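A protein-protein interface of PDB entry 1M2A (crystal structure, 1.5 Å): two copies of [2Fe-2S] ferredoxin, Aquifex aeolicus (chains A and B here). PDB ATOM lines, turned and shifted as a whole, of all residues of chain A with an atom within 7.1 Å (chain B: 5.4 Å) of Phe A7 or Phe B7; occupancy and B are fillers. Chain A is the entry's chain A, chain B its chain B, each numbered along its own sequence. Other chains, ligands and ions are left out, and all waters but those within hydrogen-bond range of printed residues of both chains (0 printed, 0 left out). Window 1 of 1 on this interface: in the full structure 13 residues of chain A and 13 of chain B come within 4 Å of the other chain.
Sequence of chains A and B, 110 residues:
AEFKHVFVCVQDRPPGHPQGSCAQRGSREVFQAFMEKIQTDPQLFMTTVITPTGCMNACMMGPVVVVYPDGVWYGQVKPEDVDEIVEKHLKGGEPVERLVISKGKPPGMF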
ATOM      1  N   HIS A   5      14.023  28.455 -29.041  1.00  0.00           N
ATOM      2  CA  HIS A   5      15.224  28.054 -29.719  1.00  0.00           C
ATOM      3  C   HIS A   5      15.583  26.695 -29.115  1.00  0.00           C
ATOM      4  O   HIS A   5      15.835  26.555 -27.900  1.00  0.00           O
ATOM      5  CB  HIS A   5      16.322  29.122 -29.420  1.00  0.00           C
ATOM      6  CG  HIS A   5      17.474  29.044 -30.357  1.00  0.00           C
ATOM      7  ND1 HIS A   5      18.329  30.103 -30.525  1.00  0.00           N
ATOM      8  CD2 HIS A   5      17.895  28.062 -31.177  1.00  0.00           C
ATOM      9  CE1 HIS A   5      19.250  29.776 -31.433  1.00  0.00           C
ATOM     10  NE2 HIS A   5      19.005  28.529 -31.838  1.00  0.00           N
ATOM     11  N   VAL A   6      15.560  25.704 -29.985  1.00  0.00           N
ATOM     12  CA  VAL A   6      15.847  24.308 -29.582  1.00  0.00           C
ATOM     13  C   VAL A   6      17.209  23.895 -29.987  1.00  0.00           C
ATOM     14  O   VAL A   6      17.555  24.149 -31.138  1.00  0.00           O
ATOM     15  CB  VAL A   6      14.823  23.377 -30.256  1.00  0.00           C
ATOM     16  CG1 VAL A   6      15.058  21.960 -29.758  1.00  0.00           C
ATOM     17  CG2 VAL A   6      13.408  23.783 -29.886  1.00  0.00           C
ATOM     18  N   PHE A   7      18.023  23.426 -29.024  1.00  0.00           N
ATOM     19  CA  PHE A   7      19.353  22.957 -29.360  1.00  0.00           C
ATOM     20  C   PHE A   7      19.399  21.467 -29.160  1.00  0.00           C
ATOM     21  O   PHE A   7      19.037  20.923 -28.108  1.00  0.00           O
ATOM     22  CB  PHE A   7      20.354  23.626 -28.444  1.00  0.00           C
ATOM     23  CG  PHE A   7      20.440  25.120 -28.663  1.00  0.00           C
ATOM     24  CD1 PHE A   7      19.646  26.029 -27.936  1.00  0.00           C
ATOM     25  CD2 PHE A   7      21.355  25.604 -29.610  1.00  0.00           C
ATOM     26  CE1 PHE A   7      19.801  27.410 -28.167  1.00  0.00           C
ATOM     27  CE2 PHE A   7      21.494  26.949 -29.827  1.00  0.00           C
ATOM     28  CZ  PHE A   7      20.746  27.866 -29.121  1.00  0.00           C
ATOM     29  N   VAL A   8      19.887  20.738 -30.161  1.00  0.00           N
ATOM     30  CA  VAL A   8      20.009  19.289 -30.122  1.00  0.00           C
ATOM     31  C   VAL A   8      21.451  18.899 -30.251  1.00  0.00           C
ATOM     32  O   VAL A   8      22.126  19.249 -31.235  1.00  0.00           O
ATOM     33  CB  VAL A   8      19.234  18.609 -31.319  1.00  0.00           C
ATOM     34  CG1 VAL A   8      19.356  17.105 -31.207  1.00  0.00           C
ATOM     35  CG2 VAL A   8      17.710  18.991 -31.266  1.00  0.00           C
ATOM     36  N   CYS A   9      21.979  18.239 -29.197  1.00  0.00           N
ATOM     37  CA  CYS A   9      23.395  17.842 -29.262  1.00  0.00           C
ATOM     38  C   CYS A   9      23.464  16.700 -30.323  1.00  0.00           C
ATOM     39  O   CYS A   9      22.743  15.710 -30.218  1.00  0.00           O
ATOM     40  CB  CYS A   9      23.809  17.278 -27.938  1.00  0.00           C
ATOM     41  SG  CYS A   9      25.536  16.599 -28.020  1.00  0.00           S
ATOM     42  N   VAL A  10      24.308  16.889 -31.343  1.00  0.00           N
ATOM     43  CA  VAL A  10      24.518  15.865 -32.387  1.00  0.00           C
ATOM     44  C   VAL A  10      25.959  15.388 -32.370  1.00  0.00           C
ATOM     45  O   VAL A  10      26.400  14.766 -33.368  1.00  0.00           O
ATOM     46  CB  VAL A  10      24.148  16.436 -33.808  1.00  0.00           C
ATOM     47  CG1 VAL A  10      22.640  16.829 -33.816  1.00  0.00           C
ATOM     48  CG2 VAL A  10      25.052  17.610 -34.172  1.00  0.00           C
ATOM     49  N   PHE A  31      17.319  15.252 -34.079  1.00  0.00           N
ATOM     50  CA  PHE A  31      17.431  16.519 -34.812  1.00  0.00           C
ATOM     51  C   PHE A  31      16.649  16.496 -36.115  1.00  0.00           C
ATOM     52  O   PHE A  31      15.887  17.424 -36.365  1.00  0.00           O
ATOM     53  CB  PHE A  31      18.920  16.809 -35.101  1.00  0.00           C
ATOM     54  CG  PHE A  31      19.156  18.097 -35.882  1.00  0.00           C
ATOM     55  CD1 PHE A  31      19.017  19.329 -35.302  1.00  0.00           C
ATOM     56  CD2 PHE A  31      19.454  18.033 -37.216  1.00  0.00           C
ATOM     57  CE1 PHE A  31      19.123  20.532 -35.998  1.00  0.00           C
ATOM     58  CE2 PHE A  31      19.587  19.201 -37.948  1.00  0.00           C
ATOM     59  CZ  PHE A  31      19.406  20.453 -37.313  1.00  0.00           C
ATOM     60  N   PHE A  34      12.933  16.858 -35.445  1.00  0.00           N
ATOM     61  CA  PHE A  34      12.569  18.222 -35.124  1.00  0.00           C
ATOM     62  C   PHE A  34      12.509  19.044 -36.403  1.00  0.00           C
ATOM     63  O   PHE A  34      11.570  19.813 -36.603  1.00  0.00           O
ATOM     64  CB  PHE A  34      13.549  18.910 -34.163  1.00  0.00           C
ATOM     65  CG  PHE A  34      13.221  18.721 -32.716  1.00  0.00           C
ATOM     66  CD1 PHE A  34      14.008  17.926 -31.889  1.00  0.00           C
ATOM     67  CD2 PHE A  34      12.134  19.370 -32.136  1.00  0.00           C
ATOM     68  CE1 PHE A  34      13.737  17.760 -30.543  1.00  0.00           C
ATOM     69  CE2 PHE A  34      11.858  19.207 -30.748  1.00  0.00           C
ATOM     70  CZ  PHE A  34      12.659  18.397 -29.948  1.00  0.00           C
ATOM     71  N   VAL A  49      13.442  27.902 -33.849  1.00  0.00           N
ATOM     72  CA  VAL A  49      14.695  27.662 -34.541  1.00  0.00           C
ATOM     73  C   VAL A  49      15.232  26.415 -33.947  1.00  0.00           C
ATOM     74  O   VAL A  49      15.107  26.263 -32.710  1.00  0.00           O
ATOM     75  CB  VAL A  49      15.715  28.748 -34.292  1.00  0.00           C
ATOM     76  CG1 VAL A  49      17.054  28.350 -34.876  1.00  0.00           C
ATOM     77  CG2 VAL A  49      15.316  30.079 -35.044  1.00  0.00           C
ATOM     78  N   ILE A  50      15.729  25.494 -34.774  1.00  0.00           N
ATOM     79  CA  ILE A  50      16.313  24.216 -34.288  1.00  0.00           C
ATOM     80  C   ILE A  50      17.777  24.236 -34.666  1.00  0.00           C
ATOM     81  O   ILE A  50      18.075  24.405 -35.862  1.00  0.00           O
ATOM     82  CB  ILE A  50      15.706  22.915 -34.971  1.00  0.00           C
ATOM     83  CG1 ILE A  50      14.192  22.915 -35.011  1.00  0.00           C
ATOM     84  CG2 ILE A  50      16.168  21.683 -34.187  1.00  0.00           C
ATOM     85  CD1 ILE A  50      13.458  22.929 -33.653  1.00  0.00           C
ATOM     86  N   THR A  51      18.699  24.090 -33.700  1.00  0.00           N
ATOM     87  CA  THR A  51      20.093  24.230 -34.012  1.00  0.00           C
ATOM     88  C   THR A  51      20.842  22.990 -33.510  1.00  0.00           C
ATOM     89  O   THR A  51      20.643  22.564 -32.376  1.00  0.00           O
ATOM     90  CB  THR A  51      20.628  25.403 -33.222  1.00  0.00           C
ATOM     91  OG1 THR A  51      19.990  26.590 -33.669  1.00  0.00           O
ATOM     92  CG2 THR A  51      22.172  25.649 -33.375  1.00  0.00           C
ATOM     93  N   PRO A  52      21.702  22.387 -34.324  1.00  0.00           N
ATOM     94  CA  PRO A  52      22.470  21.251 -33.870  1.00  0.00           C
ATOM     95  C   PRO A  52      23.705  21.747 -33.182  1.00  0.00           C
ATOM     96  O   PRO A  52      24.245  22.803 -33.533  1.00  0.00           O
ATOM     97  CB  PRO A  52      22.787  20.524 -35.189  1.00  0.00           C
ATOM     98  CG  PRO A  52      23.001  21.702 -36.131  1.00  0.00           C
ATOM     99  CD  PRO A  52      21.914  22.699 -35.724  1.00  0.00           C
ATOM    100  N   THR A  53      24.186  20.986 -32.165  1.00  0.00           N
ATOM    101  CA  THR A  53      25.313  21.454 -31.378  1.00  0.00           C
ATOM    102  C   THR A  53      26.304  20.357 -31.095  1.00  0.00           C
ATOM    103  O   THR A  53      26.003  19.167 -31.271  1.00  0.00           O
ATOM    104  CB  THR A  53      24.889  21.915 -29.953  1.00  0.00           C
ATOM    105  OG1 THR A  53      24.502  20.849 -29.098  1.00  0.00           O
ATOM    106  CG2 THR A  53      23.687  22.914 -30.024  1.00  0.00           C
ATOM    107  N   GLY A  54      27.459  20.775 -30.581  1.00  0.00           N
ATOM    108  CA  GLY A  54      28.393  19.833 -29.957  1.00  0.00           C
ATOM    109  C   GLY A  54      27.928  19.502 -28.534  1.00  0.00           C
ATOM    110  O   GLY A  54      26.964  20.041 -28.011  1.00  0.00           O
ATOM    111  N   MET A  56      26.922  19.102 -24.814  1.00  0.00           N
ATOM    112  CA  MET A  56      26.482  20.019 -23.789  1.00  0.00           C
ATOM    113  C   MET A  56      26.727  19.449 -22.389  1.00  0.00           C
ATOM    114  O   MET A  56      26.074  19.861 -21.398  1.00  0.00           O
ATOM    115  CB  MET A  56      25.004  20.453 -23.998  1.00  0.00           C
ATOM    116  CG  MET A  56      24.943  21.380 -25.278  1.00  0.00           C
ATOM    117  SD  MET A  56      23.333  22.081 -25.547  1.00  0.00           S
ATOM    118  CE  MET A  56      22.368  20.657 -26.279  1.00  0.00           C
ATOM    119  N   VAL A  64      20.583  14.825 -25.501  1.00  0.00           N
ATOM    120  CA  VAL A  64      20.304  16.040 -24.746  1.00  0.00           C
ATOM    121  C   VAL A  64      19.725  17.112 -25.719  1.00  0.00           C
ATOM    122  O   VAL A  64      20.266  17.348 -26.787  1.00  0.00           O
ATOM    123  CB  VAL A  64      21.559  16.615 -24.173  1.00  0.00           C
ATOM    124  CG1 VAL A  64      21.281  17.849 -23.435  1.00  0.00           C
ATOM    125  CG2 VAL A  64      22.174  15.561 -23.199  1.00  0.00           C
ATOM    126  N   VAL A  65      18.563  17.700 -25.334  1.00  0.00           N
ATOM    127  CA  VAL A  65      17.905  18.755 -26.091  1.00  0.00           C
ATOM    128  C   VAL A  65      17.644  19.859 -25.089  1.00  0.00           C
ATOM    129  O   VAL A  65      17.081  19.609 -24.020  1.00  0.00           O
ATOM    130  CB  VAL A  65      16.591  18.233 -26.629  1.00  0.00           C
ATOM    131  CG1 VAL A  65      15.876  19.322 -27.386  1.00  0.00           C
ATOM    132  CG2 VAL A  65      16.852  17.072 -27.617  1.00  0.00           C
ATOM    133  N   VAL A  66      17.943  21.096 -25.416  1.00  0.00           N
ATOM    134  CA  VAL A  66      17.709  22.191 -24.480  1.00  0.00           C
ATOM    135  C   VAL A  66      16.866  23.211 -25.210  1.00  0.00           C
ATOM    136  O   VAL A  66      17.151  23.554 -26.381  1.00  0.00           O
ATOM    137  CB  VAL A  66      19.016  22.816 -24.073  1.00  0.00           C
ATOM    138  CG1 VAL A  66      18.725  23.866 -23.010  1.00  0.00           C
ATOM    139  CG2 VAL A  66      19.948  21.677 -23.533  1.00  0.00           C
ATOM    140  N   VAL A  67      15.822  23.703 -24.534  1.00  0.00           N
ATOM    141  CA  VAL A  67      14.951  24.732 -25.117  1.00  0.00           C
ATOM    142  C   VAL A  67      15.094  26.060 -24.387  1.00  0.00           C
ATOM    143  O   VAL A  67      14.895  26.099 -23.148  1.00  0.00           O
ATOM    144  CB  VAL A  67      13.449  24.311 -24.993  1.00  0.00           C
ATOM    145  CG1 VAL A  67      12.572  25.322 -25.635  1.00  0.00           C
ATOM    146  CG2 VAL A  67      13.210  22.973 -25.750  1.00  0.00           C
ATOM    147  N   TYR A  68      15.435  27.110 -25.154  1.00  0.00           N
ATOM    148  CA  TYR A  68      15.609  28.428 -24.603  1.00  0.00           C
ATOM    149  C   TYR A  68      14.555  29.330 -25.246  1.00  0.00           C
ATOM    150  O   TYR A  68      14.001  29.020 -26.276  1.00  0.00           O
ATOM    151  CB  TYR A  68      17.006  28.968 -24.883  1.00  0.00           C
ATOM    152  CG  TYR A  68      18.056  28.444 -23.920  1.00  0.00           C
ATOM    153  CD1 TYR A  68      19.149  27.654 -24.357  1.00  0.00           C
ATOM    154  CD2 TYR A  68      17.922  28.687 -22.537  1.00  0.00           C
ATOM    155  CE1 TYR A  68      20.036  27.134 -23.459  1.00  0.00           C
ATOM    156  CE2 TYR A  68      18.849  28.162 -21.609  1.00  0.00           C
ATOM    157  CZ  TYR A  68      19.896  27.375 -22.085  1.00  0.00           C
ATOM    158  OH  TYR A  68      20.820  26.869 -21.232  1.00  0.00           O
ATOM    159  N   TRP A  73      15.986  21.530 -20.010  1.00  0.00           N
ATOM    160  CA  TRP A  73      16.901  20.521 -20.551  1.00  0.00           C
ATOM    161  C   TRP A  73      16.200  19.186 -20.566  1.00  0.00           C
ATOM    162  O   TRP A  73      15.644  18.754 -19.479  1.00  0.00           O
ATOM    163  CB  TRP A  73      18.125  20.385 -19.682  1.00  0.00           C
ATOM    164  CG  TRP A  73      19.015  21.559 -19.706  1.00  0.00           C
ATOM    165  CD1 TRP A  73      18.726  22.848 -19.337  1.00  0.00           C
ATOM    166  CD2 TRP A  73      20.364  21.556 -20.156  1.00  0.00           C
ATOM    167  NE1 TRP A  73      19.809  23.643 -19.550  1.00  0.00           N
ATOM    168  CE2 TRP A  73      20.838  22.882 -20.045  1.00  0.00           C
ATOM    169  CE3 TRP A  73      21.218  20.557 -20.619  1.00  0.00           C
ATOM    170  CZ2 TRP A  73      22.154  23.265 -20.393  1.00  0.00           C
ATOM    171  CZ3 TRP A  73      22.547  20.919 -20.951  1.00  0.00           C
ATOM    172  CH2 TRP A  73      23.001  22.263 -20.840  1.00  0.00           C
ATOM    173  N   HIS B   5      24.446  30.557 -20.849  1.00  0.00           N
ATOM    174  CA  HIS B   5      24.777  29.503 -21.801  1.00  0.00           C
ATOM    175  C   HIS B   5      25.120  30.222 -23.083  1.00  0.00           C
ATOM    176  O   HIS B   5      24.300  30.952 -23.649  1.00  0.00           O
ATOM    177  CB  HIS B   5      23.536  28.570 -21.998  1.00  0.00           C
ATOM    178  CG  HIS B   5      23.900  27.255 -22.584  1.00  0.00           C
ATOM    179  ND1 HIS B   5      23.090  26.145 -22.462  1.00  0.00           N
ATOM    180  CD2 HIS B   5      24.970  26.877 -23.329  1.00  0.00           C
ATOM    181  CE1 HIS B   5      23.643  25.126 -23.118  1.00  0.00           C
ATOM    182  NE2 HIS B   5      24.797  25.553 -23.649  1.00  0.00           N
ATOM    183  N   VAL B   6      26.384  30.102 -23.506  1.00  0.00           N
ATOM    184  CA  VAL B   6      26.846  30.811 -24.693  1.00  0.00           C
ATOM    185  C   VAL B   6      26.988  29.826 -25.844  1.00  0.00           C
ATOM    186  O   VAL B   6      27.620  28.800 -25.688  1.00  0.00           O
ATOM    187  CB  VAL B   6      28.293  31.379 -24.426  1.00  0.00           C
ATOM    188  CG1 VAL B   6      28.802  32.195 -25.609  1.00  0.00           C
ATOM    189  CG2 VAL B   6      28.209  32.280 -23.214  1.00  0.00           C
ATOM    190  N   PHE B   7      26.408  30.171 -26.980  1.00  0.00           N
ATOM    191  CA  PHE B   7      26.450  29.309 -28.151  1.00  0.00           C
ATOM    192  C   PHE B   7      27.201  30.021 -29.215  1.00  0.00           C
ATOM    193  O   PHE B   7      26.882  31.177 -29.554  1.00  0.00           O
ATOM    194  CB  PHE B   7      25.017  29.055 -28.632  1.00  0.00           C
ATOM    195  CG  PHE B   7      24.260  28.205 -27.655  1.00  0.00           C
ATOM    196  CD1 PHE B   7      23.424  28.786 -26.699  1.00  0.00           C
ATOM    197  CD2 PHE B   7      24.329  26.819 -27.787  1.00  0.00           C
ATOM    198  CE1 PHE B   7      22.642  27.935 -25.880  1.00  0.00           C
ATOM    199  CE2 PHE B   7      23.523  25.944 -26.962  1.00  0.00           C
ATOM    200  CZ  PHE B   7      22.682  26.518 -26.022  1.00  0.00           C
ATOM    201  N   VAL B   8      28.256  29.396 -29.765  1.00  0.00           N
ATOM    202  CA  VAL B   8      29.089  29.973 -30.822  1.00  0.00           C
ATOM    203  C   VAL B   8      28.928  29.119 -32.071  1.00  0.00           C
ATOM    204  O   VAL B   8      29.198  27.922 -32.053  1.00  0.00           O
ATOM    205  CB  VAL B   8      30.581  29.972 -30.355  1.00  0.00           C
ATOM    206  CG1 VAL B   8      31.460  30.558 -31.453  1.00  0.00           C
ATOM    207  CG2 VAL B   8      30.778  30.705 -29.004  1.00  0.00           C
ATOM    208  N   CYS B   9      28.521  29.759 -33.148  1.00  0.00           N
ATOM    209  CA  CYS B   9      28.326  29.005 -34.407  1.00  0.00           C
ATOM    210  C   CYS B   9      29.782  28.738 -34.906  1.00  0.00           C
ATOM    211  O   CYS B   9      30.593  29.675 -35.075  1.00  0.00           O
ATOM    212  CB  CYS B   9      27.606  29.880 -35.403  1.00  0.00           C
ATOM    213  SG  CYS B   9      27.540  29.045 -37.054  1.00  0.00           S
ATOM    214  N   THR B  51      29.045  26.359 -25.830  1.00  0.00           N
ATOM    215  CA  THR B  51      28.700  25.277 -26.703  1.00  0.00           C
ATOM    216  C   THR B  51      28.890  25.659 -28.144  1.00  0.00           C
ATOM    217  O   THR B  51      28.438  26.683 -28.559  1.00  0.00           O
ATOM    218  CB  THR B  51      27.193  24.893 -26.489  1.00  0.00           C
ATOM    219  OG1 THR B  51      26.945  24.550 -25.118  1.00  0.00           O
ATOM    220  CG2 THR B  51      26.769  23.725 -27.342  1.00  0.00           C
ATOM    221  N   THR B  53      28.117  25.323 -32.165  1.00  0.00           N
ATOM    222  CA  THR B  53      26.907  24.919 -32.854  1.00  0.00           C
ATOM    223  C   THR B  53      27.081  24.950 -34.343  1.00  0.00           C
ATOM    224  O   THR B  53      28.053  25.502 -34.871  1.00  0.00           O
ATOM    225  CB  THR B  53      25.735  25.914 -32.580  1.00  0.00           C
ATOM    226  OG1 THR B  53      25.960  27.153 -33.280  1.00  0.00           O
ATOM    227  CG2 THR B  53      25.558  26.164 -31.042  1.00  0.00           C
ATOM    228  N   MET B  56      23.202  29.237 -37.232  1.00  0.00           N
ATOM    229  CA  MET B  56      22.043  29.782 -36.549  1.00  0.00           C
ATOM    230  C   MET B  56      21.342  30.824 -37.411  1.00  0.00           C
ATOM    231  O   MET B  56      20.638  31.717 -36.904  1.00  0.00           O
ATOM    232  CB  MET B  56      22.490  30.359 -35.213  1.00  0.00           C
ATOM    233  CG  MET B  56      22.736  29.172 -34.191  1.00  0.00           C
ATOM    234  SD  MET B  56      23.035  29.681 -32.487  1.00  0.00           S
ATOM    235  CE  MET B  56      24.764  30.374 -32.534  1.00  0.00           C
ATOM    236  N   VAL B  64      28.598  34.551 -35.249  1.00  0.00           N
ATOM    237  CA  VAL B  64      27.395  34.733 -34.454  1.00  0.00           C
ATOM    238  C   VAL B  64      27.565  33.993 -33.120  1.00  0.00           C
ATOM    239  O   VAL B  64      27.969  32.832 -33.041  1.00  0.00           O
ATOM    240  CB  VAL B  64      26.215  34.124 -35.154  1.00  0.00           C
ATOM    241  CG1 VAL B  64      24.920  34.259 -34.352  1.00  0.00           C
ATOM    242  CG2 VAL B  64      26.041  34.875 -36.561  1.00  0.00           C
ATOM    243  N   VAL B  65      27.242  34.709 -32.018  1.00  0.00           N
ATOM    244  CA  VAL B  65      27.314  34.146 -30.665  1.00  0.00           C
ATOM    245  C   VAL B  65      25.992  34.520 -30.004  1.00  0.00           C
ATOM    246  O   VAL B  65      25.545  35.674 -30.069  1.00  0.00           O
ATOM    247  CB  VAL B  65      28.455  34.861 -29.915  1.00  0.00           C
ATOM    248  CG1 VAL B  65      28.558  34.335 -28.486  1.00  0.00           C
ATOM    249  CG2 VAL B  65      29.830  34.562 -30.645  1.00  0.00           C
ATOM    250  N   VAL B  66      25.330  33.588 -29.360  1.00  0.00           N
ATOM    251  CA  VAL B  66      24.037  33.877 -28.711  1.00  0.00           C
ATOM    252  C   VAL B  66      24.176  33.525 -27.255  1.00  0.00           C
ATOM    253  O   VAL B  66      24.718  32.443 -26.949  1.00  0.00           O
ATOM    254  CB  VAL B  66      22.952  33.004 -29.326  1.00  0.00           C
ATOM    255  CG1 VAL B  66      21.654  33.486 -28.751  1.00  0.00           C
ATOM    256  CG2 VAL B  66      22.962  33.250 -30.826  1.00  0.00           C
ATOM    257  N   VAL B  67      23.647  34.375 -26.358  1.00  0.00           N
ATOM    258  CA  VAL B  67      23.786  34.110 -24.907  1.00  0.00           C
ATOM    259  C   VAL B  67      22.362  33.907 -24.368  1.00  0.00           C
ATOM    260  O   VAL B  67      21.496  34.822 -24.550  1.00  0.00           O
ATOM    261  CB  VAL B  67      24.402  35.320 -24.188  1.00  0.00           C
ATOM    262  CG1 VAL B  67      24.493  35.000 -22.714  1.00  0.00           C
ATOM    263  CG2 VAL B  67      25.850  35.568 -24.727  1.00  0.00           C
ATOM    264  N   TYR B  68      22.148  32.754 -23.758  1.00  0.00           N
ATOM    265  CA  TYR B  68      20.870  32.427 -23.160  1.00  0.00           C
ATOM    266  C   TYR B  68      21.049  32.294 -21.685  1.00  0.00           C
ATOM    267  O   TYR B  68      22.134  32.094 -21.212  1.00  0.00           O
ATOM    268  CB  TYR B  68      20.354  31.120 -23.805  1.00  0.00           C
ATOM    269  CG  TYR B  68      19.628  31.356 -25.117  1.00  0.00           C
ATOM    270  CD1 TYR B  68      20.093  30.741 -26.300  1.00  0.00           C
ATOM    271  CD2 TYR B  68      18.522  32.222 -25.225  1.00  0.00           C
ATOM    272  CE1 TYR B  68      19.505  30.977 -27.506  1.00  0.00           C
ATOM    273  CE2 TYR B  68      17.891  32.488 -26.414  1.00  0.00           C
ATOM    274  CZ  TYR B  68      18.390  31.861 -27.577  1.00  0.00           C
ATOM    275  OH  TYR B  68      17.788  32.084 -28.748  1.00  0.00           O
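ND1 of His A5 sits at hydrogen-bond distance from OH of Tyr B68 (2.7 Å). The side-chain hydroxyl (OH) of Tyr A68 lies within hydrogen-bond range of a ring nitrogen (ND1) of His B5 (2.7 Å).
The backbone NH of Thr A51 sits at hydrogen-bond distance from the backbone carbonyl oxygen of Val A6, at 2.8 Å. The backbone NH (N) of Phe A7 is in hydrogen-bond range of the backbone carbonyl oxygen (O) of Val A66, at 2.8 Å. N of Val A8 sits at hydrogen-bond distance from O of Thr A51. The side-chain sulfur (SG) of Cys A9 lies close to the backbone carbonyl oxygen (O) of Gly A54 (3.7 Å). OG1 of Thr B51 is in hydrogen-bond range of NE2 of His B5 (2.8 Å). The backbone carbonyl oxygen of Val B8 is in hydrogen-bond range of the backbone NH of Thr B53, at 2.8 Å.
Among the printed residues, pairs that only touch across the chains: Phe A7 with Phe B7 (3.4 Å), Pro A52 with Thr B53 (3.5 Å), Tyr A68 with Tyr B68 (3.5 Å), Met A56 with Thr B51 (3.6 Å), Trp A73 with His B5 (3.6 Å), Phe A7 with Tyr B68 (3.6 Å), Tyr A68 with Phe B7 (3.6 Å), Thr A51 with Met B56 (3.7 Å), Thr A51 with Thr B53 (3.7 Å), Thr A53 with Thr B51 (3.7 Å), Gly A54 with Thr B51 (3.7 Å), Thr A53 with Thr B53 (3.9 Å), Met A56 with His B5 (3.9 Å) and His A5 with Met B56 (3.9 Å).
Phe A7 touches just these residues of chain B: Phe B7 (3.4 Å) and Tyr B68 (3.6 Å). Of the printed residues of chain A, Thr B53 touches Thr A51 (3.7 Å), Pro A52 (3.5 Å) and Thr A53 (3.9 Å). Printed residues of chain A within 4 Å of Met B56: His A5 (3.9 Å) and Thr A51 (3.7 Å). Of the printed residues of chain B, Thr A53 touches Thr B51 and Thr B53. Of the printed residues of chain B, His A5 touches Met B56 and Tyr B68.
Of the 13 printed residues of chain B, 6 touch a printed residue of chain A. Of the 21 printed residues of chain A, 9 touch a printed residue of chain B. Along chain A the printed residues that touch a printed residue of chain B span positions 5 to 73.
His A5 touches Met B56, and with the chains exchanged Met A56 touches His B5. His A5 touches Tyr B68, and with the chains exchanged Tyr A68 touches His B5. Thr A51 touches Thr B53, and with the chains exchanged Thr A53 touches Thr B51. Thr A53 touches its own counterpart, Thr B53.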
